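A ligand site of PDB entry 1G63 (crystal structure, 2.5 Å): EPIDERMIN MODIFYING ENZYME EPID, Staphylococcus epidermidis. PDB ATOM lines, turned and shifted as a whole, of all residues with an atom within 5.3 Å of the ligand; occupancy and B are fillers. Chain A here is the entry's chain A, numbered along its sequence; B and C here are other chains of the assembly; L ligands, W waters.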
ATOM      1  N   THR A  10     -17.429 -32.964 -13.707  1.00  0.00           N
ATOM      2  CA  THR A  10     -17.141 -31.667 -13.125  1.00  0.00           C
ATOM      3  C   THR A  10     -17.037 -30.582 -14.200  1.00  0.00           C
ATOM      4  O   THR A  10     -16.994 -30.876 -15.400  1.00  0.00           O
ATOM      5  CB  THR A  10     -15.853 -31.723 -12.291  1.00  0.00           C
ATOM      6  OG1 THR A  10     -14.721 -31.967 -13.139  1.00  0.00           O
ATOM      7  CG2 THR A  10     -15.956 -32.846 -11.258  1.00  0.00           C
ATOM      8  N   ALA A  11     -16.977 -29.331 -13.743  1.00  0.00           N
ATOM      9  CA  ALA A  11     -16.923 -28.163 -14.615  1.00  0.00           C
ATOM     10  C   ALA A  11     -15.678 -27.980 -15.495  1.00  0.00           C
ATOM     11  O   ALA A  11     -14.981 -26.963 -15.430  1.00  0.00           O
ATOM     12  CB  ALA A  11     -17.146 -26.913 -13.774  1.00  0.00           C
ATOM     13  N   SER A  12     -15.416 -28.993 -16.309  1.00  0.00           N
ATOM     14  CA  SER A  12     -14.304 -28.967 -17.239  1.00  0.00           C
ATOM     15  C   SER A  12     -14.967 -28.701 -18.581  1.00  0.00           C
ATOM     16  O   SER A  12     -16.080 -29.174 -18.815  1.00  0.00           O
ATOM     17  CB  SER A  12     -13.600 -30.313 -17.281  1.00  0.00           C
ATOM     18  OG  SER A  12     -12.904 -30.476 -18.504  1.00  0.00           O
ATOM     19  N   ILE A  13     -14.285 -27.962 -19.445  1.00  0.00           N
ATOM     20  CA  ILE A  13     -14.834 -27.643 -20.761  1.00  0.00           C
ATOM     21  C   ILE A  13     -15.280 -28.901 -21.523  1.00  0.00           C
ATOM     22  O   ILE A  13     -16.253 -28.873 -22.275  1.00  0.00           O
ATOM     23  CB  ILE A  13     -13.806 -26.869 -21.622  1.00  0.00           C
ATOM     24  CG1 ILE A  13     -14.420 -26.489 -22.970  1.00  0.00           C
ATOM     25  CG2 ILE A  13     -12.538 -27.702 -21.797  1.00  0.00           C
ATOM     26  CD1 ILE A  13     -15.690 -25.654 -22.868  1.00  0.00           C
ATOM     27  N   ASN A  14     -14.579 -30.003 -21.304  1.00  0.00           N
ATOM     28  CA  ASN A  14     -14.919 -31.242 -21.979  1.00  0.00           C
ATOM     29  C   ASN A  14     -16.158 -31.956 -21.463  1.00  0.00           C
ATOM     30  O   ASN A  14     -16.530 -33.007 -21.984  1.00  0.00           O
ATOM     31  CB  ASN A  14     -13.740 -32.204 -21.969  1.00  0.00           C
ATOM     32  CG  ASN A  14     -12.620 -31.750 -22.889  1.00  0.00           C
ATOM     33  OD1 ASN A  14     -11.556 -31.323 -22.444  1.00  0.00           O
ATOM     34  ND2 ASN A  14     -12.863 -31.823 -24.192  1.00  0.00           N
ATOM     35  N   SER A  37     -21.447 -31.764 -11.010  1.00  0.00           N
ATOM     36  CA  SER A  37     -21.086 -30.804  -9.994  1.00  0.00           C
ATOM     37  C   SER A  37     -21.943 -29.569 -10.289  1.00  0.00           C
ATOM     38  O   SER A  37     -22.306 -29.322 -11.438  1.00  0.00           O
ATOM     39  CB  SER A  37     -19.605 -30.443 -10.089  1.00  0.00           C
ATOM     40  OG  SER A  37     -19.341 -29.602 -11.202  1.00  0.00           O
ATOM     41  N   PRO A  38     -22.311 -28.800  -9.274  1.00  0.00           N
ATOM     42  CA  PRO A  38     -23.143 -27.609  -9.518  1.00  0.00           C
ATOM     43  C   PRO A  38     -22.630 -26.729 -10.671  1.00  0.00           C
ATOM     44  O   PRO A  38     -23.406 -26.305 -11.514  1.00  0.00           O
ATOM     45  CB  PRO A  38     -23.099 -26.890  -8.182  1.00  0.00           C
ATOM     46  CG  PRO A  38     -23.064 -28.037  -7.206  1.00  0.00           C
ATOM     47  CD  PRO A  38     -22.033 -28.962  -7.834  1.00  0.00           C
ATOM     48  N   SER A  39     -21.326 -26.470 -10.688  1.00  0.00           N
ATOM     49  CA  SER A  39     -20.744 -25.622 -11.713  1.00  0.00           C
ATOM     50  C   SER A  39     -20.805 -26.168 -13.130  1.00  0.00           C
ATOM     51  O   SER A  39     -20.850 -25.407 -14.103  1.00  0.00           O
ATOM     52  CB  SER A  39     -19.282 -25.305 -11.366  1.00  0.00           C
ATOM     53  OG  SER A  39     -19.185 -24.565 -10.163  1.00  0.00           O
ATOM     54  N   SER A  40     -20.808 -27.488 -13.272  1.00  0.00           N
ATOM     55  CA  SER A  40     -20.845 -28.067 -14.605  1.00  0.00           C
ATOM     56  C   SER A  40     -22.166 -27.781 -15.302  1.00  0.00           C
ATOM     57  O   SER A  40     -22.271 -27.892 -16.525  1.00  0.00           O
ATOM     58  CB  SER A  40     -20.561 -29.574 -14.541  1.00  0.00           C
ATOM     59  OG  SER A  40     -21.473 -30.242 -13.704  1.00  0.00           O
ATOM     60  N   PHE A  43     -22.316 -25.359 -18.221  1.00  0.00           N
ATOM     61  CA  PHE A  43     -21.757 -25.741 -19.508  1.00  0.00           C
ATOM     62  C   PHE A  43     -22.731 -26.534 -20.364  1.00  0.00           C
ATOM     63  O   PHE A  43     -22.661 -26.493 -21.588  1.00  0.00           O
ATOM     64  CB  PHE A  43     -20.508 -26.596 -19.314  1.00  0.00           C
ATOM     65  CG  PHE A  43     -19.363 -25.874 -18.672  1.00  0.00           C
ATOM     66  CD1 PHE A  43     -19.463 -25.416 -17.360  1.00  0.00           C
ATOM     67  CD2 PHE A  43     -18.181 -25.686 -19.358  1.00  0.00           C
ATOM     68  CE1 PHE A  43     -18.390 -24.773 -16.753  1.00  0.00           C
ATOM     69  CE2 PHE A  43     -17.103 -25.048 -18.758  1.00  0.00           C
ATOM     70  CZ  PHE A  43     -17.210 -24.589 -17.452  1.00  0.00           C
ATOM     71  N   ALA A  82     -12.289 -34.671 -14.697  1.00  0.00           N
ATOM     72  CA  ALA A  82     -11.992 -34.280 -13.316  1.00  0.00           C
ATOM     73  C   ALA A  82     -11.245 -32.946 -13.290  1.00  0.00           C
ATOM     74  O   ALA A  82     -10.138 -32.832 -13.819  1.00  0.00           O
ATOM     75  CB  ALA A  82     -11.162 -35.368 -12.623  1.00  0.00           C
ATOM     76  N   SER A  83     -11.865 -31.944 -12.674  1.00  0.00           N
ATOM     77  CA  SER A  83     -11.276 -30.606 -12.576  1.00  0.00           C
ATOM     78  C   SER A  83     -10.224 -30.540 -11.484  1.00  0.00           C
ATOM     79  O   SER A  83     -10.208 -31.360 -10.559  1.00  0.00           O
ATOM     80  CB  SER A  83     -12.362 -29.580 -12.272  1.00  0.00           C
ATOM     81  OG  SER A  83     -12.984 -29.858 -11.033  1.00  0.00           O
ATOM     82  N   ALA A  84      -9.333 -29.570 -11.592  1.00  0.00           N
ATOM     83  CA  ALA A  84      -8.296 -29.381 -10.585  1.00  0.00           C
ATOM     84  C   ALA A  84      -8.995 -29.162  -9.234  1.00  0.00           C
ATOM     85  O   ALA A  84      -8.590 -29.724  -8.210  1.00  0.00           O
ATOM     86  CB  ALA A  84      -7.447 -28.180 -10.930  1.00  0.00           C
ATOM     87  N   ASN A  85     -10.045 -28.359  -9.253  1.00  0.00           N
ATOM     88  CA  ASN A  85     -10.809 -28.057  -8.049  1.00  0.00           C
ATOM     89  C   ASN A  85     -11.346 -29.288  -7.312  1.00  0.00           C
ATOM     90  O   ASN A  85     -11.158 -29.417  -6.099  1.00  0.00           O
ATOM     91  CB  ASN A  85     -11.966 -27.117  -8.369  1.00  0.00           C
ATOM     92  CG  ASN A  85     -12.839 -26.821  -7.151  1.00  0.00           C
ATOM     93  OD1 ASN A  85     -14.018 -27.161  -7.132  1.00  0.00           O
ATOM     94  ND2 ASN A  85     -12.260 -26.207  -6.131  1.00  0.00           N
ATOM     95  N   THR A  86     -12.027 -30.176  -8.036  1.00  0.00           N
ATOM     96  CA  THR A  86     -12.575 -31.362  -7.395  1.00  0.00           C
ATOM     97  C   THR A  86     -11.478 -32.332  -6.940  1.00  0.00           C
ATOM     98  O   THR A  86     -11.569 -32.952  -5.880  1.00  0.00           O
ATOM     99  CB  THR A  86     -13.586 -32.068  -8.337  1.00  0.00           C
ATOM    100  OG1 THR A  86     -14.803 -31.314  -8.352  1.00  0.00           O
ATOM    101  CG2 THR A  86     -13.905 -33.495  -7.859  1.00  0.00           C
ATOM    102  N   LYS A  89     -10.240 -31.005  -3.758  1.00  0.00           N
ATOM    103  CA  LYS A  89     -11.225 -31.148  -2.683  1.00  0.00           C
ATOM    104  C   LYS A  89     -11.210 -32.607  -2.176  1.00  0.00           C
ATOM    105  O   LYS A  89     -11.197 -32.870  -0.975  1.00  0.00           O
ATOM    106  CB  LYS A  89     -12.628 -30.809  -3.179  1.00  0.00           C
ATOM    107  CG  LYS A  89     -12.957 -29.337  -3.278  1.00  0.00           C
ATOM    108  CD  LYS A  89     -14.397 -29.166  -3.735  1.00  0.00           C
ATOM    109  CE  LYS A  89     -14.893 -27.751  -3.570  1.00  0.00           C
ATOM    110  NZ  LYS A  89     -16.312 -27.688  -3.991  1.00  0.00           N
ATOM    111  N   ASN A  97     -20.671 -30.752  -1.788  1.00  0.00           N
ATOM    112  CA  ASN A  97     -21.736 -30.938  -2.760  1.00  0.00           C
ATOM    113  C   ASN A  97     -21.922 -32.451  -2.891  1.00  0.00           C
ATOM    114  O   ASN A  97     -21.107 -33.221  -2.379  1.00  0.00           O
ATOM    115  CB  ASN A  97     -21.434 -30.268  -4.107  1.00  0.00           C
ATOM    116  CG  ASN A  97     -20.124 -30.733  -4.715  1.00  0.00           C
ATOM    117  OD1 ASN A  97     -19.791 -31.909  -4.685  1.00  0.00           O
ATOM    118  ND2 ASN A  97     -19.386 -29.791  -5.304  1.00  0.00           N
ATOM    119  N   ASN A 115      -8.464 -33.308 -16.246  1.00  0.00           N
ATOM    120  CA  ASN A 115      -8.597 -32.565 -17.493  1.00  0.00           C
ATOM    121  C   ASN A 115      -8.567 -31.086 -17.150  1.00  0.00           C
ATOM    122  O   ASN A 115      -9.428 -30.587 -16.410  1.00  0.00           O
ATOM    123  CB  ASN A 115      -9.889 -32.881 -18.232  1.00  0.00           C
ATOM    124  CG  ASN A 115      -9.956 -32.173 -19.579  1.00  0.00           C
ATOM    125  OD1 ASN A 115     -10.714 -31.230 -19.765  1.00  0.00           O
ATOM    126  ND2 ASN A 115      -9.126 -32.625 -20.516  1.00  0.00           N
ATOM    127  N   MET A 116      -7.568 -30.391 -17.692  1.00  0.00           N
ATOM    128  CA  MET A 116      -7.397 -28.969 -17.464  1.00  0.00           C
ATOM    129  C   MET A 116      -6.288 -28.476 -18.392  1.00  0.00           C
ATOM    130  O   MET A 116      -5.599 -29.272 -19.024  1.00  0.00           O
ATOM    131  CB  MET A 116      -6.975 -28.722 -16.020  1.00  0.00           C
ATOM    132  CG  MET A 116      -5.667 -29.418 -15.645  1.00  0.00           C
ATOM    133  SD  MET A 116      -5.271 -29.416 -13.874  1.00  0.00           S
ATOM    134  CE  MET A 116      -6.218 -30.848 -13.347  1.00  0.00           C
ATOM    135  N   ASN A 117      -6.131 -27.155 -18.455  1.00  0.00           N
ATOM    136  CA  ASN A 117      -5.098 -26.575 -19.286  1.00  0.00           C
ATOM    137  C   ASN A 117      -3.759 -26.964 -18.686  1.00  0.00           C
ATOM    138  O   ASN A 117      -3.655 -27.127 -17.465  1.00  0.00           O
ATOM    139  CB  ASN A 117      -5.249 -25.052 -19.326  1.00  0.00           C
ATOM    140  CG  ASN A 117      -4.201 -24.386 -20.194  1.00  0.00           C
ATOM    141  OD1 ASN A 117      -3.057 -24.202 -19.773  1.00  0.00           O
ATOM    142  ND2 ASN A 117      -4.593 -24.041 -21.420  1.00  0.00           N
ATOM    143  N   MET A 120      -2.425 -25.180 -15.509  1.00  0.00           N
ATOM    144  CA  MET A 120      -3.064 -25.508 -14.233  1.00  0.00           C
ATOM    145  C   MET A 120      -2.476 -26.804 -13.713  1.00  0.00           C
ATOM    146  O   MET A 120      -2.301 -26.986 -12.501  1.00  0.00           O
ATOM    147  CB  MET A 120      -4.580 -25.692 -14.417  1.00  0.00           C
ATOM    148  CG  MET A 120      -5.339 -24.445 -14.836  1.00  0.00           C
ATOM    149  SD  MET A 120      -7.103 -24.771 -15.104  1.00  0.00           S
ATOM    150  CE  MET A 120      -7.653 -25.048 -13.421  1.00  0.00           C
ATOM    151  N   PRO B  63     -20.584 -16.158 -16.578  1.00  0.00           N
ATOM    152  CA  PRO B  63     -20.180 -17.429 -15.965  1.00  0.00           C
ATOM    153  C   PRO B  63     -19.106 -18.226 -16.711  1.00  0.00           C
ATOM    154  O   PRO B  63     -18.518 -19.141 -16.154  1.00  0.00           O
ATOM    155  CB  PRO B  63     -21.500 -18.206 -15.884  1.00  0.00           C
ATOM    156  CG  PRO B  63     -22.533 -17.150 -15.832  1.00  0.00           C
ATOM    157  CD  PRO B  63     -22.031 -16.172 -16.851  1.00  0.00           C
ATOM    158  N   LEU B  64     -18.851 -17.872 -17.975  1.00  0.00           N
ATOM    159  CA  LEU B  64     -17.859 -18.580 -18.771  1.00  0.00           C
ATOM    160  C   LEU B  64     -16.590 -17.774 -19.063  1.00  0.00           C
ATOM    161  O   LEU B  64     -15.980 -17.931 -20.125  1.00  0.00           O
ATOM    162  CB  LEU B  64     -18.468 -19.064 -20.089  1.00  0.00           C
ATOM    163  CG  LEU B  64     -19.591 -20.120 -20.052  1.00  0.00           C
ATOM    164  CD1 LEU B  64     -19.180 -21.261 -19.146  1.00  0.00           C
ATOM    165  CD2 LEU B  64     -20.886 -19.491 -19.537  1.00  0.00           C
ATOM    166  N   LEU B  65     -16.193 -16.930 -18.122  1.00  0.00           N
ATOM    167  CA  LEU B  65     -14.995 -16.106 -18.266  1.00  0.00           C
ATOM    168  C   LEU B  65     -13.762 -17.022 -18.350  1.00  0.00           C
ATOM    169  O   LEU B  65     -13.644 -17.992 -17.599  1.00  0.00           O
ATOM    170  CB  LEU B  65     -14.894 -15.175 -17.056  1.00  0.00           C
ATOM    171  CG  LEU B  65     -14.723 -13.659 -17.263  1.00  0.00           C
ATOM    172  CD1 LEU B  65     -15.288 -13.221 -18.605  1.00  0.00           C
ATOM    173  CD2 LEU B  65     -15.409 -12.944 -16.118  1.00  0.00           C
ATOM    174  N   HIS B  67     -10.413 -17.931 -17.395  1.00  0.00           N
ATOM    175  CA  HIS B  67      -9.412 -17.664 -16.356  1.00  0.00           C
ATOM    176  C   HIS B  67      -7.970 -17.751 -16.862  1.00  0.00           C
ATOM    177  O   HIS B  67      -7.080 -17.080 -16.332  1.00  0.00           O
ATOM    178  CB  HIS B  67      -9.619 -18.624 -15.188  1.00  0.00           C
ATOM    179  CG  HIS B  67      -9.568 -20.071 -15.583  1.00  0.00           C
ATOM    180  ND1 HIS B  67      -8.418 -20.837 -15.465  1.00  0.00           N
ATOM    181  CD2 HIS B  67     -10.501 -20.873 -16.148  1.00  0.00           C
ATOM    182  CE1 HIS B  67      -8.657 -22.042 -15.937  1.00  0.00           C
ATOM    183  NE2 HIS B  67      -9.913 -22.093 -16.361  1.00  0.00           N
ATOM    184  N   CYS B  95     -10.185 -24.357  -5.810  1.00  0.00           N
ATOM    185  CA  CYS B  95     -10.575 -23.281  -6.698  1.00  0.00           C
ATOM    186  C   CYS B  95     -12.047 -23.415  -7.086  1.00  0.00           C
ATOM    187  O   CYS B  95     -12.383 -23.750  -8.222  1.00  0.00           O
ATOM    188  CB  CYS B  95      -9.672 -23.265  -7.934  1.00  0.00           C
ATOM    189  SG  CYS B  95      -9.233 -24.898  -8.562  1.00  0.00           S
ATOM    190  N   ASP B  96     -12.935 -23.107  -6.141  1.00  0.00           N
ATOM    191  CA  ASP B  96     -14.375 -23.214  -6.357  1.00  0.00           C
ATOM    192  C   ASP B  96     -15.111 -21.939  -6.794  1.00  0.00           C
ATOM    193  O   ASP B  96     -16.336 -21.913  -6.828  1.00  0.00           O
ATOM    194  CB  ASP B  96     -15.058 -23.814  -5.113  1.00  0.00           C
ATOM    195  CG  ASP B  96     -14.754 -23.033  -3.839  1.00  0.00           C
ATOM    196  OD1 ASP B  96     -14.134 -21.956  -3.899  1.00  0.00           O
ATOM    197  OD2 ASP B  96     -15.161 -23.522  -2.766  1.00  0.00           O
ATOM    198  N   ASN B  97     -14.360 -20.885  -7.101  1.00  0.00           N
ATOM    199  CA  ASN B  97     -14.933 -19.646  -7.625  1.00  0.00           C
ATOM    200  C   ASN B  97     -13.887 -19.060  -8.593  1.00  0.00           C
ATOM    201  O   ASN B  97     -12.750 -19.521  -8.617  1.00  0.00           O
ATOM    202  CB  ASN B  97     -15.297 -18.651  -6.501  1.00  0.00           C
ATOM    203  CG  ASN B  97     -14.129 -18.295  -5.594  1.00  0.00           C
ATOM    204  OD1 ASN B  97     -12.998 -18.116  -6.069  1.00  0.00           O
ATOM    205  ND2 ASN B  97     -14.399 -18.177  -4.297  1.00  0.00           N
ATOM    206  N   THR B 101      -9.858 -19.683  -8.757  1.00  0.00           N
ATOM    207  CA  THR B 101      -9.406 -20.464  -9.917  1.00  0.00           C
ATOM    208  C   THR B 101      -8.274 -19.694 -10.619  1.00  0.00           C
ATOM    209  O   THR B 101      -7.337 -20.290 -11.166  1.00  0.00           O
ATOM    210  CB  THR B 101     -10.551 -20.714 -10.927  1.00  0.00           C
ATOM    211  OG1 THR B 101     -11.516 -21.595 -10.356  1.00  0.00           O
ATOM    212  CG2 THR B 101     -10.010 -21.344 -12.205  1.00  0.00           C
ATOM    213  N   LEU C  51     -18.001 -20.321 -27.157  1.00  0.00           N
ATOM    214  CA  LEU C  51     -16.602 -20.708 -27.025  1.00  0.00           C
ATOM    215  C   LEU C  51     -16.027 -21.277 -28.309  1.00  0.00           C
ATOM    216  O   LEU C  51     -14.815 -21.398 -28.441  1.00  0.00           O
ATOM    217  CB  LEU C  51     -16.449 -21.735 -25.885  1.00  0.00           C
ATOM    218  CG  LEU C  51     -16.891 -21.255 -24.501  1.00  0.00           C
ATOM    219  CD1 LEU C  51     -16.921 -22.416 -23.532  1.00  0.00           C
ATOM    220  CD2 LEU C  51     -15.950 -20.161 -24.012  1.00  0.00           C
HETATM  221  N1  LIG L   1     -11.234 -26.301 -14.707  1.00  0.00           N
HETATM  222  C1  LIG L   1     -10.556 -27.480 -14.902  1.00  0.00           C
HETATM  223  O1  LIG L   1     -10.035 -28.111 -14.031  1.00  0.00           O
HETATM  224  N2  LIG L   1     -10.470 -28.003 -16.218  1.00  0.00           N
HETATM  225  C2  LIG L   1     -10.998 -27.437 -17.331  1.00  0.00           C
HETATM  226  O2  LIG L   1     -10.833 -27.968 -18.432  1.00  0.00           O
HETATM  227  C3  LIG L   1     -11.691 -26.154 -17.136  1.00  0.00           C
HETATM  228  N3  LIG L   1     -12.280 -25.532 -18.147  1.00  0.00           N
HETATM  229  C4  LIG L   1     -13.048 -24.442 -17.908  1.00  0.00           C
HETATM  230  C5  LIG L   1     -13.785 -23.813 -18.997  1.00  0.00           C
HETATM  231  C6  LIG L   1     -14.468 -22.638 -18.860  1.00  0.00           C
HETATM  232  C7  LIG L   1     -15.250 -22.012 -20.036  1.00  0.00           C
HETATM  233  C8  LIG L   1     -14.695 -22.094 -17.501  1.00  0.00           C
HETATM  234  C9  LIG L   1     -15.557 -20.884 -17.272  1.00  0.00           C
HETATM  235  C10 LIG L   1     -13.977 -22.666 -16.450  1.00  0.00           C
HETATM  236  C11 LIG L   1     -13.156 -23.814 -16.597  1.00  0.00           C
HETATM  237  N4  LIG L   1     -12.440 -24.446 -15.547  1.00  0.00           N
HETATM  238  C12 LIG L   1     -11.776 -25.651 -15.734  1.00  0.00           C
HETATM  239  C13 LIG L   1     -12.512 -23.902 -14.179  1.00  0.00           C
HETATM  240  C14 LIG L   1     -13.609 -24.649 -13.386  1.00  0.00           C
HETATM  241  O3  LIG L   1     -14.920 -24.582 -13.976  1.00  0.00           O
HETATM  242  C15 LIG L   1     -13.700 -24.100 -11.964  1.00  0.00           C
HETATM  243  O4  LIG L   1     -12.437 -24.300 -11.284  1.00  0.00           O
HETATM  244  C16 LIG L   1     -14.816 -24.656 -11.095  1.00  0.00           C
HETATM  245  O5  LIG L   1     -14.924 -23.922  -9.860  1.00  0.00           O
HETATM  246  C17 LIG L   1     -14.693 -26.150 -10.798  1.00  0.00           C
HETATM  247  O6  LIG L   1     -15.853 -26.614 -10.082  1.00  0.00           O
HETATM  248  P1  LIG L   1     -16.208 -28.136  -9.914  1.00  0.00           P
HETATM  249  O7  LIG L   1     -15.048 -28.783  -9.280  1.00  0.00           O
HETATM  250  O8  LIG L   1     -16.570 -28.713 -11.247  1.00  0.00           O
HETATM  251  O9  LIG L   1     -17.480 -28.130  -8.977  1.00  0.00           O
HETATM  252  O   HOH W   1     -19.673 -26.905  -8.453  1.00  0.00           O
HETATM  253  O   HOH W   2      -8.714 -28.252 -20.150  1.00  0.00           O
HETATM  254  O   HOH W   3     -16.988 -29.792  -6.961  1.00  0.00           O
HETATM  255  O   HOH W   4     -16.848 -26.706  -6.298  1.00  0.00           O
HETATM  256  O   HOH W   5     -16.054 -21.346 -10.233  1.00  0.00           O
HETATM  257  O   HOH W   6     -10.862 -26.616 -11.354  1.00  0.00           O
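Thr 10 touches the ligand (CB to O8, 3.3 Å). Ser 39 touches the ligand (CB to O6, 3.9 Å). Phe 43 touches the ligand. Met 116 touches the ligand (CA to N2, 3.5 Å). Met 120 touches the ligand. Pro 63 of chain B touches the ligand (O to C9, 3.6 Å). CA of Leu 64 of chain B touches C9 of the ligand (3.6 Å). Leu 65 of chain B touches the ligand (O to C9, 3.5 Å). His 67 of chain B touches the ligand (NE2 to N4, 3.5 Å). Asp 96 of chain B touches the ligand. Leu 51 of chain C touches the ligand. Hydrophobic or aromatic side chains within 4 Å of the ligand: Ala 11, Ile 13, Phe 43, Met 116, Met 120, His 67 of chain B and Leu 51 of chain C.
An oxygen (O3) of the ligand lies within hydrogen-bond range of the backbone carbonyl oxygen (O) of Ala 11 (2.8 Å). The backbone NH of Ile 13 sits at hydrogen-bond distance from a nitrogen (N3) of the ligand (3.4 Å). The backbone carbonyl oxygen (O) of Asn 115 sits at hydrogen-bond distance from a nitrogen (N2) of the ligand. The side-chain amide oxygen (OD1) of Asn 85 lies close to an oxygen (O7) of the ligand (2.9 Å). OG of Ser 12 is in hydrogen-bond range of O2 of the ligand (3.3 Å). O8 of the ligand sits at hydrogen-bond distance from N of Ala 11. The side-chain hydroxyl (OG1) of Thr 101 of chain B is in hydrogen-bond range of an oxygen (O4) of the ligand, 3.0 Å away. The side-chain hydroxyl of Ser 37 lies within hydrogen-bond range of an oxygen (O8) of the ligand, at 2.9 Å. OG of Ser 83 lies within hydrogen-bond range of O7 of the ligand. O of Cys 95 of chain B is in hydrogen-bond range of O5 of the ligand, 3.0 Å away. An oxygen (O1) of the ligand is in hydrogen-bond range of the backbone NH (N) of Ala 84, at 2.9 Å. The side-chain hydroxyl of Thr 86 lies within hydrogen-bond range of an oxygen (O7) of the ligand (2.7 Å).
N of Asp 96 of chain B lies close to ND2 of Asn 85 (3.2 Å). The backbone carbonyl oxygen of Ala 82 is in hydrogen-bond range of the backbone NH of Asn 115 (3.0 Å). The side-chain amide nitrogen (ND2) of Asn 85 sits close to the backbone NH (N) of Cys 95 of chain B, 2.8 Å away. O of Cys 95 of chain B lies within hydrogen-bond range of OG1 of Thr 101 of chain B, at 3.2 Å. The side-chain hydroxyl of Thr 101 of chain B sits at hydrogen-bond distance from the backbone carbonyl oxygen of Asn 97 of chain B (3.0 Å). OG of Ser 12 lies within hydrogen-bond range of OD1 of Asn 115 (2.6 Å). The backbone NH (N) of Ala 11 sits at hydrogen-bond distance from the side-chain hydroxyl (OG) of Ser 37. The side-chain amide oxygen (OD1) of Asn 115 lies close to the side-chain amide oxygen (OD1) of Asn 14 (2.8 Å).
Water W1 lies within hydrogen-bond range of O9 of the ligand (2.6 Å) and N of Ser 39 (2.8 Å). Water W3 lies within hydrogen-bond range of an oxygen (O9) of the ligand (2.7 Å), the side-chain amide nitrogen (ND2) of Asn 97 of chain A (2.9 Å) and the side-chain hydroxyl (OG1) of Thr 86 (3.0 Å). Water W2 lies within hydrogen-bond range of an oxygen (O2) of the ligand, the backbone NH (N) of Asn 117 and the backbone NH (N) of Met 116. Water W6 lies within hydrogen-bond range of O4 of the ligand (2.8 Å), N of Asn 85 (2.8 Å), N of Ala 84 (3.3 Å) and SG of Cys 95 of chain B (3.7 Å). Water W5 lies within hydrogen-bond range of O5 of the ligand (2.8 Å) and O of Asp 96 of chain B (3.5 Å). Water W4 lies within hydrogen-bond range of the side-chain amino group of Lys 89, the side-chain amide oxygen of Asn 85 and an oxygen (O9) of the ligand.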
